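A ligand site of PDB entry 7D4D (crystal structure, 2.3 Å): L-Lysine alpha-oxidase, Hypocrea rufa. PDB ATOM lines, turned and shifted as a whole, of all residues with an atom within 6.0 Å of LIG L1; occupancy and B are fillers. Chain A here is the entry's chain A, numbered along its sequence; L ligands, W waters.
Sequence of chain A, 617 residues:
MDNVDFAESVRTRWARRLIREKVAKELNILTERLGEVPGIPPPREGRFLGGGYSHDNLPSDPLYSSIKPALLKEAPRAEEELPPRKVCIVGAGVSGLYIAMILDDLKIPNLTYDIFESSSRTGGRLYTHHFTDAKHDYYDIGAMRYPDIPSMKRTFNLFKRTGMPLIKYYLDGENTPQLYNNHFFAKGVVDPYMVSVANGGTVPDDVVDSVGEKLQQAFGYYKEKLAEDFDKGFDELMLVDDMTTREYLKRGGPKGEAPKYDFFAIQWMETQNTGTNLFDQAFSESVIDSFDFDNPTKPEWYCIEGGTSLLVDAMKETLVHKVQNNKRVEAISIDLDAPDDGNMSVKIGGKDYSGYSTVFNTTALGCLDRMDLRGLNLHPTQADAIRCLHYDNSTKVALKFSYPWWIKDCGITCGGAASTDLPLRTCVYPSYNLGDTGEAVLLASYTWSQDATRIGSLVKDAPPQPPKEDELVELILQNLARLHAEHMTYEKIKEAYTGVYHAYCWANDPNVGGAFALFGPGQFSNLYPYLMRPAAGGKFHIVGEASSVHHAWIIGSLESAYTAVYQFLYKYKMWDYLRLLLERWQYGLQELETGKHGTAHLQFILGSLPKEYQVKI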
ATOM      1  N   MET A 144     -32.304  10.206   7.650  1.00  0.00           N
ATOM      2  CA  MET A 144     -33.715   9.842   7.560  1.00  0.00           C
ATOM      3  C   MET A 144     -34.679  10.763   8.305  1.00  0.00           C
ATOM      4  O   MET A 144     -35.859  10.773   7.959  1.00  0.00           O
ATOM      5  CB  MET A 144     -33.944   8.404   8.031  1.00  0.00           C
ATOM      6  CG  MET A 144     -33.608   8.178   9.498  1.00  0.00           C
ATOM      7  SD  MET A 144     -33.521   6.424  10.029  1.00  0.00           S
ATOM      8  CE  MET A 144     -35.270   5.961  10.016  1.00  0.00           C
ATOM      9  N   ARG A 145     -34.242  11.546   9.304  1.00  0.00           N
ATOM     10  CA  ARG A 145     -35.162  12.240  10.188  1.00  0.00           C
ATOM     11  C   ARG A 145     -34.610  13.624  10.546  1.00  0.00           C
ATOM     12  O   ARG A 145     -33.401  13.817  10.666  1.00  0.00           O
ATOM     13  CB  ARG A 145     -35.422  11.431  11.452  1.00  0.00           C
ATOM     14  CG  ARG A 145     -34.170  11.192  12.254  1.00  0.00           C
ATOM     15  CD  ARG A 145     -34.401  10.204  13.358  1.00  0.00           C
ATOM     16  NE  ARG A 145     -33.145   9.706  13.886  1.00  0.00           N
ATOM     17  CZ  ARG A 145     -33.045   8.700  14.748  1.00  0.00           C
ATOM     18  NH1 ARG A 145     -34.142   8.092  15.175  1.00  0.00           N
ATOM     19  NH2 ARG A 145     -31.851   8.304  15.169  1.00  0.00           N
ATOM     20  N   LEU A 278     -19.540   4.694  23.507  1.00  0.00           N
ATOM     21  CA  LEU A 278     -19.487   6.061  22.988  1.00  0.00           C
ATOM     22  C   LEU A 278     -19.310   7.131  24.063  1.00  0.00           C
ATOM     23  O   LEU A 278     -18.975   8.268  23.726  1.00  0.00           O
ATOM     24  CB  LEU A 278     -20.734   6.365  22.134  1.00  0.00           C
ATOM     25  CG  LEU A 278     -20.694   5.758  20.718  1.00  0.00           C
ATOM     26  CD1 LEU A 278     -21.913   6.162  19.868  1.00  0.00           C
ATOM     27  CD2 LEU A 278     -19.362   6.101  19.993  1.00  0.00           C
ATOM     28  N   ASP A 289     -25.568  15.693  21.092  1.00  0.00           N
ATOM     29  CA  ASP A 289     -26.525  14.667  20.692  1.00  0.00           C
ATOM     30  C   ASP A 289     -27.752  14.668  21.601  1.00  0.00           C
ATOM     31  O   ASP A 289     -28.882  14.445  21.136  1.00  0.00           O
ATOM     32  CB  ASP A 289     -25.864  13.285  20.689  1.00  0.00           C
ATOM     33  CG  ASP A 289     -25.057  13.015  19.419  1.00  0.00           C
ATOM     34  OD1 ASP A 289     -25.051  13.885  18.509  1.00  0.00           O
ATOM     35  OD2 ASP A 289     -24.427  11.931  19.337  1.00  0.00           O
ATOM     36  N   PHE A 293     -31.527  15.148  20.036  1.00  0.00           N
ATOM     37  CA  PHE A 293     -32.512  14.085  20.177  1.00  0.00           C
ATOM     38  C   PHE A 293     -33.481  14.317  21.329  1.00  0.00           C
ATOM     39  O   PHE A 293     -34.567  13.726  21.350  1.00  0.00           O
ATOM     40  CB  PHE A 293     -31.807  12.729  20.351  1.00  0.00           C
ATOM     41  CG  PHE A 293     -31.336  12.139  19.053  1.00  0.00           C
ATOM     42  CD1 PHE A 293     -32.226  11.498  18.202  1.00  0.00           C
ATOM     43  CD2 PHE A 293     -29.999  12.216  18.679  1.00  0.00           C
ATOM     44  CE1 PHE A 293     -31.797  10.959  16.990  1.00  0.00           C
ATOM     45  CE2 PHE A 293     -29.557  11.674  17.477  1.00  0.00           C
ATOM     46  CZ  PHE A 293     -30.458  11.055  16.628  1.00  0.00           C
ATOM     47  N   TRP A 301     -40.576  15.978  14.643  1.00  0.00           N
ATOM     48  CA  TRP A 301     -39.634  15.459  13.672  1.00  0.00           C
ATOM     49  C   TRP A 301     -40.346  15.204  12.356  1.00  0.00           C
ATOM     50  O   TRP A 301     -41.545  14.896  12.339  1.00  0.00           O
ATOM     51  CB  TRP A 301     -38.974  14.160  14.166  1.00  0.00           C
ATOM     52  CG  TRP A 301     -38.182  14.349  15.420  1.00  0.00           C
ATOM     53  CD1 TRP A 301     -38.665  14.604  16.662  1.00  0.00           C
ATOM     54  CD2 TRP A 301     -36.756  14.295  15.546  1.00  0.00           C
ATOM     55  NE1 TRP A 301     -37.631  14.726  17.556  1.00  0.00           N
ATOM     56  CE2 TRP A 301     -36.449  14.539  16.889  1.00  0.00           C
ATOM     57  CE3 TRP A 301     -35.707  14.072  14.633  1.00  0.00           C
ATOM     58  CZ2 TRP A 301     -35.136  14.552  17.357  1.00  0.00           C
ATOM     59  CZ3 TRP A 301     -34.403  14.099  15.107  1.00  0.00           C
ATOM     60  CH2 TRP A 301     -34.128  14.337  16.448  1.00  0.00           C
ATOM     61  N   ASP A 392     -17.365   7.747  13.812  1.00  0.00           N
ATOM     62  CA  ASP A 392     -18.235   6.700  14.335  1.00  0.00           C
ATOM     63  C   ASP A 392     -18.735   5.824  13.193  1.00  0.00           C
ATOM     64  O   ASP A 392     -18.872   6.274  12.058  1.00  0.00           O
ATOM     65  CB  ASP A 392     -19.437   7.316  15.069  1.00  0.00           C
ATOM     66  CG  ASP A 392     -20.220   6.296  15.901  1.00  0.00           C
ATOM     67  OD1 ASP A 392     -19.643   5.261  16.314  1.00  0.00           O
ATOM     68  OD2 ASP A 392     -21.424   6.524  16.155  1.00  0.00           O
ATOM     69  N   TYR A 446     -30.648  -0.707  13.591  1.00  0.00           N
ATOM     70  CA  TYR A 446     -29.938   0.550  13.407  1.00  0.00           C
ATOM     71  C   TYR A 446     -28.934   0.618  14.544  1.00  0.00           C
ATOM     72  O   TYR A 446     -29.331   0.639  15.717  1.00  0.00           O
ATOM     73  CB  TYR A 446     -30.904   1.731  13.399  1.00  0.00           C
ATOM     74  CG  TYR A 446     -30.252   3.076  13.163  1.00  0.00           C
ATOM     75  CD1 TYR A 446     -28.979   3.161  12.619  1.00  0.00           C
ATOM     76  CD2 TYR A 446     -30.899   4.256  13.523  1.00  0.00           C
ATOM     77  CE1 TYR A 446     -28.353   4.386  12.425  1.00  0.00           C
ATOM     78  CE2 TYR A 446     -30.290   5.498  13.346  1.00  0.00           C
ATOM     79  CZ  TYR A 446     -29.015   5.562  12.804  1.00  0.00           C
ATOM     80  OH  TYR A 446     -28.399   6.786  12.613  1.00  0.00           O
ATOM     81  N   TRP A 448     -24.724   1.770  15.998  1.00  0.00           N
ATOM     82  CA  TRP A 448     -23.621   2.712  15.975  1.00  0.00           C
ATOM     83  C   TRP A 448     -22.378   2.028  16.548  1.00  0.00           C
ATOM     84  O   TRP A 448     -22.488   1.033  17.271  1.00  0.00           O
ATOM     85  CB  TRP A 448     -23.907   3.964  16.841  1.00  0.00           C
ATOM     86  CG  TRP A 448     -24.879   4.951  16.285  1.00  0.00           C
ATOM     87  CD1 TRP A 448     -25.182   5.162  14.987  1.00  0.00           C
ATOM     88  CD2 TRP A 448     -25.664   5.878  17.045  1.00  0.00           C
ATOM     89  NE1 TRP A 448     -26.117   6.159  14.869  1.00  0.00           N
ATOM     90  CE2 TRP A 448     -26.430   6.611  16.119  1.00  0.00           C
ATOM     91  CE3 TRP A 448     -25.786   6.163  18.412  1.00  0.00           C
ATOM     92  CZ2 TRP A 448     -27.318   7.619  16.520  1.00  0.00           C
ATOM     93  CZ3 TRP A 448     -26.664   7.158  18.807  1.00  0.00           C
ATOM     94  CH2 TRP A 448     -27.425   7.882  17.862  1.00  0.00           C
ATOM     95  N   PHE A 516     -19.833   9.151  10.234  1.00  0.00           N
ATOM     96  CA  PHE A 516     -19.858  10.589  10.441  1.00  0.00           C
ATOM     97  C   PHE A 516     -18.899  10.918  11.560  1.00  0.00           C
ATOM     98  O   PHE A 516     -18.549  10.043  12.368  1.00  0.00           O
ATOM     99  CB  PHE A 516     -21.260  11.116  10.773  1.00  0.00           C
ATOM    100  CG  PHE A 516     -22.070  10.191  11.637  1.00  0.00           C
ATOM    101  CD1 PHE A 516     -21.690   9.931  12.947  1.00  0.00           C
ATOM    102  CD2 PHE A 516     -23.232   9.615  11.154  1.00  0.00           C
ATOM    103  CE1 PHE A 516     -22.447   9.072  13.747  1.00  0.00           C
ATOM    104  CE2 PHE A 516     -24.001   8.759  11.943  1.00  0.00           C
ATOM    105  CZ  PHE A 516     -23.602   8.486  13.245  1.00  0.00           C
ATOM    106  N   ALA A 517     -18.437  12.164  11.581  1.00  0.00           N
ATOM    107  CA  ALA A 517     -17.532  12.616  12.626  1.00  0.00           C
ATOM    108  C   ALA A 517     -18.160  12.417  13.997  1.00  0.00           C
ATOM    109  O   ALA A 517     -19.360  12.606  14.179  1.00  0.00           O
ATOM    110  CB  ALA A 517     -17.176  14.077  12.422  1.00  0.00           C
ATOM    111  N   LEU A 518     -17.340  12.006  14.942  1.00  0.00           N
ATOM    112  CA  LEU A 518     -17.762  11.991  16.345  1.00  0.00           C
ATOM    113  C   LEU A 518     -16.458  12.143  17.124  1.00  0.00           C
ATOM    114  O   LEU A 518     -15.744  11.154  17.347  1.00  0.00           O
ATOM    115  CB  LEU A 518     -18.537  10.738  16.721  1.00  0.00           C
ATOM    116  CG  LEU A 518     -19.332  10.782  18.042  1.00  0.00           C
ATOM    117  CD1 LEU A 518     -20.525   9.816  18.029  1.00  0.00           C
ATOM    118  CD2 LEU A 518     -18.446  10.470  19.222  1.00  0.00           C
ATOM    119  N   HIS A 551     -22.133  17.736  13.629  1.00  0.00           N
ATOM    120  CA  HIS A 551     -21.768  16.439  13.070  1.00  0.00           C
ATOM    121  C   HIS A 551     -22.994  15.565  12.902  1.00  0.00           C
ATOM    122  O   HIS A 551     -23.929  15.593  13.704  1.00  0.00           O
ATOM    123  CB  HIS A 551     -20.760  15.740  13.979  1.00  0.00           C
ATOM    124  CG  HIS A 551     -19.452  16.451  14.121  1.00  0.00           C
ATOM    125  ND1 HIS A 551     -18.611  16.250  15.183  1.00  0.00           N
ATOM    126  CD2 HIS A 551     -18.843  17.352  13.318  1.00  0.00           C
ATOM    127  CE1 HIS A 551     -17.520  16.982  15.040  1.00  0.00           C
ATOM    128  NE2 HIS A 551     -17.634  17.658  13.906  1.00  0.00           N
ATOM    129  N   ALA A 552     -22.984  14.774  11.830  1.00  0.00           N
ATOM    130  CA  ALA A 552     -23.972  13.731  11.555  1.00  0.00           C
ATOM    131  C   ALA A 552     -25.376  14.292  11.308  1.00  0.00           C
ATOM    132  O   ALA A 552     -26.369  13.555  11.432  1.00  0.00           O
ATOM    133  CB  ALA A 552     -24.011  12.683  12.676  1.00  0.00           C
ATOM    134  N   TRP A 553     -25.456  15.571  10.943  1.00  0.00           N
ATOM    135  CA  TRP A 553     -26.691  16.238  10.522  1.00  0.00           C
ATOM    136  C   TRP A 553     -26.450  16.972   9.212  1.00  0.00           C
ATOM    137  O   TRP A 553     -25.365  17.509   8.973  1.00  0.00           O
ATOM    138  CB  TRP A 553     -27.187  17.234  11.579  1.00  0.00           C
ATOM    139  CG  TRP A 553     -27.566  16.567  12.844  1.00  0.00           C
ATOM    140  CD1 TRP A 553     -26.850  16.540  14.008  1.00  0.00           C
ATOM    141  CD2 TRP A 553     -28.766  15.812  13.086  1.00  0.00           C
ATOM    142  NE1 TRP A 553     -27.512  15.807  14.960  1.00  0.00           N
ATOM    143  CE2 TRP A 553     -28.691  15.362  14.426  1.00  0.00           C
ATOM    144  CE3 TRP A 553     -29.884  15.491  12.319  1.00  0.00           C
ATOM    145  CZ2 TRP A 553     -29.712  14.574  15.004  1.00  0.00           C
ATOM    146  CZ3 TRP A 553     -30.895  14.717  12.899  1.00  0.00           C
ATOM    147  CH2 TRP A 553     -30.793  14.263  14.223  1.00  0.00           C
HETATM  148  N1  LIG L   1     -28.026  12.280  12.855  1.00  0.00           N
HETATM  149  C1  LIG L   1     -27.948  10.832  13.024  1.00  0.00           C
HETATM  150  C2  LIG L   1     -29.301  10.242  13.462  1.00  0.00           C
HETATM  151  O1  LIG L   1     -30.356  10.881  13.386  1.00  0.00           O
HETATM  152  C3  LIG L   1     -26.848  10.480  14.024  1.00  0.00           C
HETATM  153  C4  LIG L   1     -26.909  11.297  15.305  1.00  0.00           C
HETATM  154  C5  LIG L   1     -25.872  10.853  16.328  1.00  0.00           C
HETATM  155  C6  LIG L   1     -24.488  11.298  15.911  1.00  0.00           C
HETATM  156  N2  LIG L   1     -23.452  10.887  16.890  1.00  0.00           N
HETATM  157  O2  LIG L   1     -29.379   9.103  13.920  1.00  0.00           O
HETATM  158  P1  LG2 L   2     -20.915  13.198   1.940  1.00  0.00           P
HETATM  159  O1  LG2 L   2     -19.995  12.085   2.310  1.00  0.00           O
HETATM  160  O2  LG2 L   2     -22.376  12.803   1.975  1.00  0.00           O
HETATM  161  O3  LG2 L   2     -20.464  13.726   0.528  1.00  0.00           O
HETATM  162  C1  LG2 L   2     -19.109  13.556   0.062  1.00  0.00           C
HETATM  163  C2  LG2 L   2     -19.125  12.966  -1.328  1.00  0.00           C
HETATM  164  O4  LG2 L   2     -17.781  12.908  -1.860  1.00  0.00           O
HETATM  165  C3  LG2 L   2     -19.695  11.547  -1.434  1.00  0.00           C
HETATM  166  O5  LG2 L   2     -20.707  11.509  -2.432  1.00  0.00           O
HETATM  167  C4  LG2 L   2     -18.474  10.689  -1.799  1.00  0.00           C
HETATM  168  O6  LG2 L   2     -18.808   9.618  -2.682  1.00  0.00           O
HETATM  169  C5  LG2 L   2     -17.632  11.698  -2.566  1.00  0.00           C
HETATM  170  N1  LG2 L   2     -16.199  11.393  -2.659  1.00  0.00           N
HETATM  171  C6  LG2 L   2     -15.445  10.717  -1.730  1.00  0.00           C
HETATM  172  N2  LG2 L   2     -14.179  10.591  -2.048  1.00  0.00           N
HETATM  173  C7  LG2 L   2     -14.086  11.246  -3.265  1.00  0.00           C
HETATM  174  C8  LG2 L   2     -13.001  11.478  -4.128  1.00  0.00           C
HETATM  175  N3  LG2 L   2     -11.756  11.066  -3.875  1.00  0.00           N
HETATM  176  N4  LG2 L   2     -13.243  12.159  -5.272  1.00  0.00           N
HETATM  177  C9  LG2 L   2     -14.486  12.576  -5.516  1.00  0.00           C
HETATM  178  N5  LG2 L   2     -15.583  12.426  -4.772  1.00  0.00           N
HETATM  179  C10 LG2 L   2     -15.316  11.750  -3.648  1.00  0.00           C
HETATM  180  N6  LG2 L   2     -28.487  13.865   8.997  1.00  0.00           N
HETATM  181  C11 LG2 L   2     -29.718  14.368   9.353  1.00  0.00           C
HETATM  182  O7  LG2 L   2     -29.994  15.568   9.260  1.00  0.00           O
HETATM  183  N7  LG2 L   2     -30.697  13.487   9.835  1.00  0.00           N
HETATM  184  C12 LG2 L   2     -30.555  12.122   9.987  1.00  0.00           C
HETATM  185  O8  LG2 L   2     -31.483  11.429  10.416  1.00  0.00           O
HETATM  186  C13 LG2 L   2     -29.253  11.605   9.624  1.00  0.00           C
HETATM  187  N8  LG2 L   2     -29.051  10.321   9.737  1.00  0.00           N
HETATM  188  C14 LG2 L   2     -27.805   9.823   9.362  1.00  0.00           C
HETATM  189  C15 LG2 L   2     -27.564   8.453   9.495  1.00  0.00           C
HETATM  190  C16 LG2 L   2     -26.348   7.899   9.114  1.00  0.00           C
HETATM  191  C17 LG2 L   2     -26.128   6.422   9.268  1.00  0.00           C
HETATM  192  C18 LG2 L   2     -25.331   8.741   8.611  1.00  0.00           C
HETATM  193  C19 LG2 L   2     -23.994   8.179   8.219  1.00  0.00           C
HETATM  194  C20 LG2 L   2     -25.565  10.104   8.505  1.00  0.00           C
HETATM  195  C21 LG2 L   2     -26.783  10.653   8.878  1.00  0.00           C
HETATM  196  N9  LG2 L   2     -27.056  12.039   8.743  1.00  0.00           N
HETATM  197  C22 LG2 L   2     -28.292  12.551   9.118  1.00  0.00           C
HETATM  198  C23 LG2 L   2     -26.011  12.967   8.324  1.00  0.00           C
HETATM  199  C24 LG2 L   2     -26.043  13.340   6.854  1.00  0.00           C
HETATM  200  O9  LG2 L   2     -26.466  12.239   6.069  1.00  0.00           O
HETATM  201  C25 LG2 L   2     -24.630  13.797   6.471  1.00  0.00           C
HETATM  202  O10 LG2 L   2     -24.159  14.698   7.461  1.00  0.00           O
HETATM  203  C26 LG2 L   2     -24.519  14.477   5.128  1.00  0.00           C
HETATM  204  O11 LG2 L   2     -25.367  13.806   4.191  1.00  0.00           O
HETATM  205  C27 LG2 L   2     -23.072  14.516   4.692  1.00  0.00           C
HETATM  206  O12 LG2 L   2     -22.944  15.327   3.516  1.00  0.00           O
HETATM  207  P2  LG2 L   2     -21.544  15.789   3.001  1.00  0.00           P
HETATM  208  O13 LG2 L   2     -20.955  16.646   4.123  1.00  0.00           O
HETATM  209  O14 LG2 L   2     -21.665  16.358   1.660  1.00  0.00           O
HETATM  210  O15 LG2 L   2     -20.701  14.418   2.939  1.00  0.00           O
HETATM  211  O   HOH W   1     -21.613  12.660  15.695  1.00  0.00           O
HETATM  212  O   HOH W   2     -23.362   7.979  16.797  1.00  0.00           O
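Water W1 lies within hydrogen-bond range of O of Ala 517 (2.7 Å) and N2 of LIG L1 (2.8 Å). Water W2 lies within hydrogen-bond range of the side-chain carboxylate (OD2) of Asp 392 and a nitrogen (N2) of LIG L1.
The backbone NH (N) of Asp 392 lies within hydrogen-bond range of the backbone carbonyl oxygen (O) of Phe 516, 3.0 Å away. The indole nitrogen (NE1) of Trp 448 is in hydrogen-bond range of the side-chain hydroxyl (OH) of Tyr 446 (3.3 Å).
The side-chain hydroxyl of Tyr 446 sits at hydrogen-bond distance from an oxygen (O2) of LIG L1, 2.8 Å away. A nitrogen (N1) of LIG L1 is in hydrogen-bond range of the backbone carbonyl oxygen (O) of Ala 552 (2.5 Å). O10 of LG2 L2 is in hydrogen-bond range of O of Trp 553 (3.4 Å). The backbone carbonyl oxygen of Arg 145 is in hydrogen-bond range of a nitrogen (N7) of LG2 L2. The backbone NH (N) of Arg 145 lies within hydrogen-bond range of an oxygen (O8) of LG2 L2 (3.0 Å). The backbone NH (N) of Met 144 sits at hydrogen-bond distance from an oxygen (O8) of LG2 L2 (3.1 Å). The side-chain carboxylate of Asp 289 is in salt-bridge range of a nitrogen (N2) of LIG L1, 2.8 Å away. The guanidinium group (NH2) of Arg 145 is in salt-bridge range of an oxygen (O2) of LIG L1.
Residues that only touch LIG L1: Phe 293 (3.2 Å), Trp 448 (3.5 Å), Phe 516 (3.7 Å), Leu 518 (3.3 Å) and Trp 553 (3.5 Å). Hydrophobic or aromatic side chains that line LIG L1: Phe 293, Tyr 446, Trp 448, Phe 516, Leu 518, Ala 552 and Trp 553. Nine residues have an atom within 4 Å of LIG L1: Arg 145, Asp 289, Phe 293, Tyr 446, Trp 448, Phe 516, Leu 518, Ala 552 and Trp 553. The nearest printed residue that does not touch LIG L1 is His 551 (4.9 Å).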
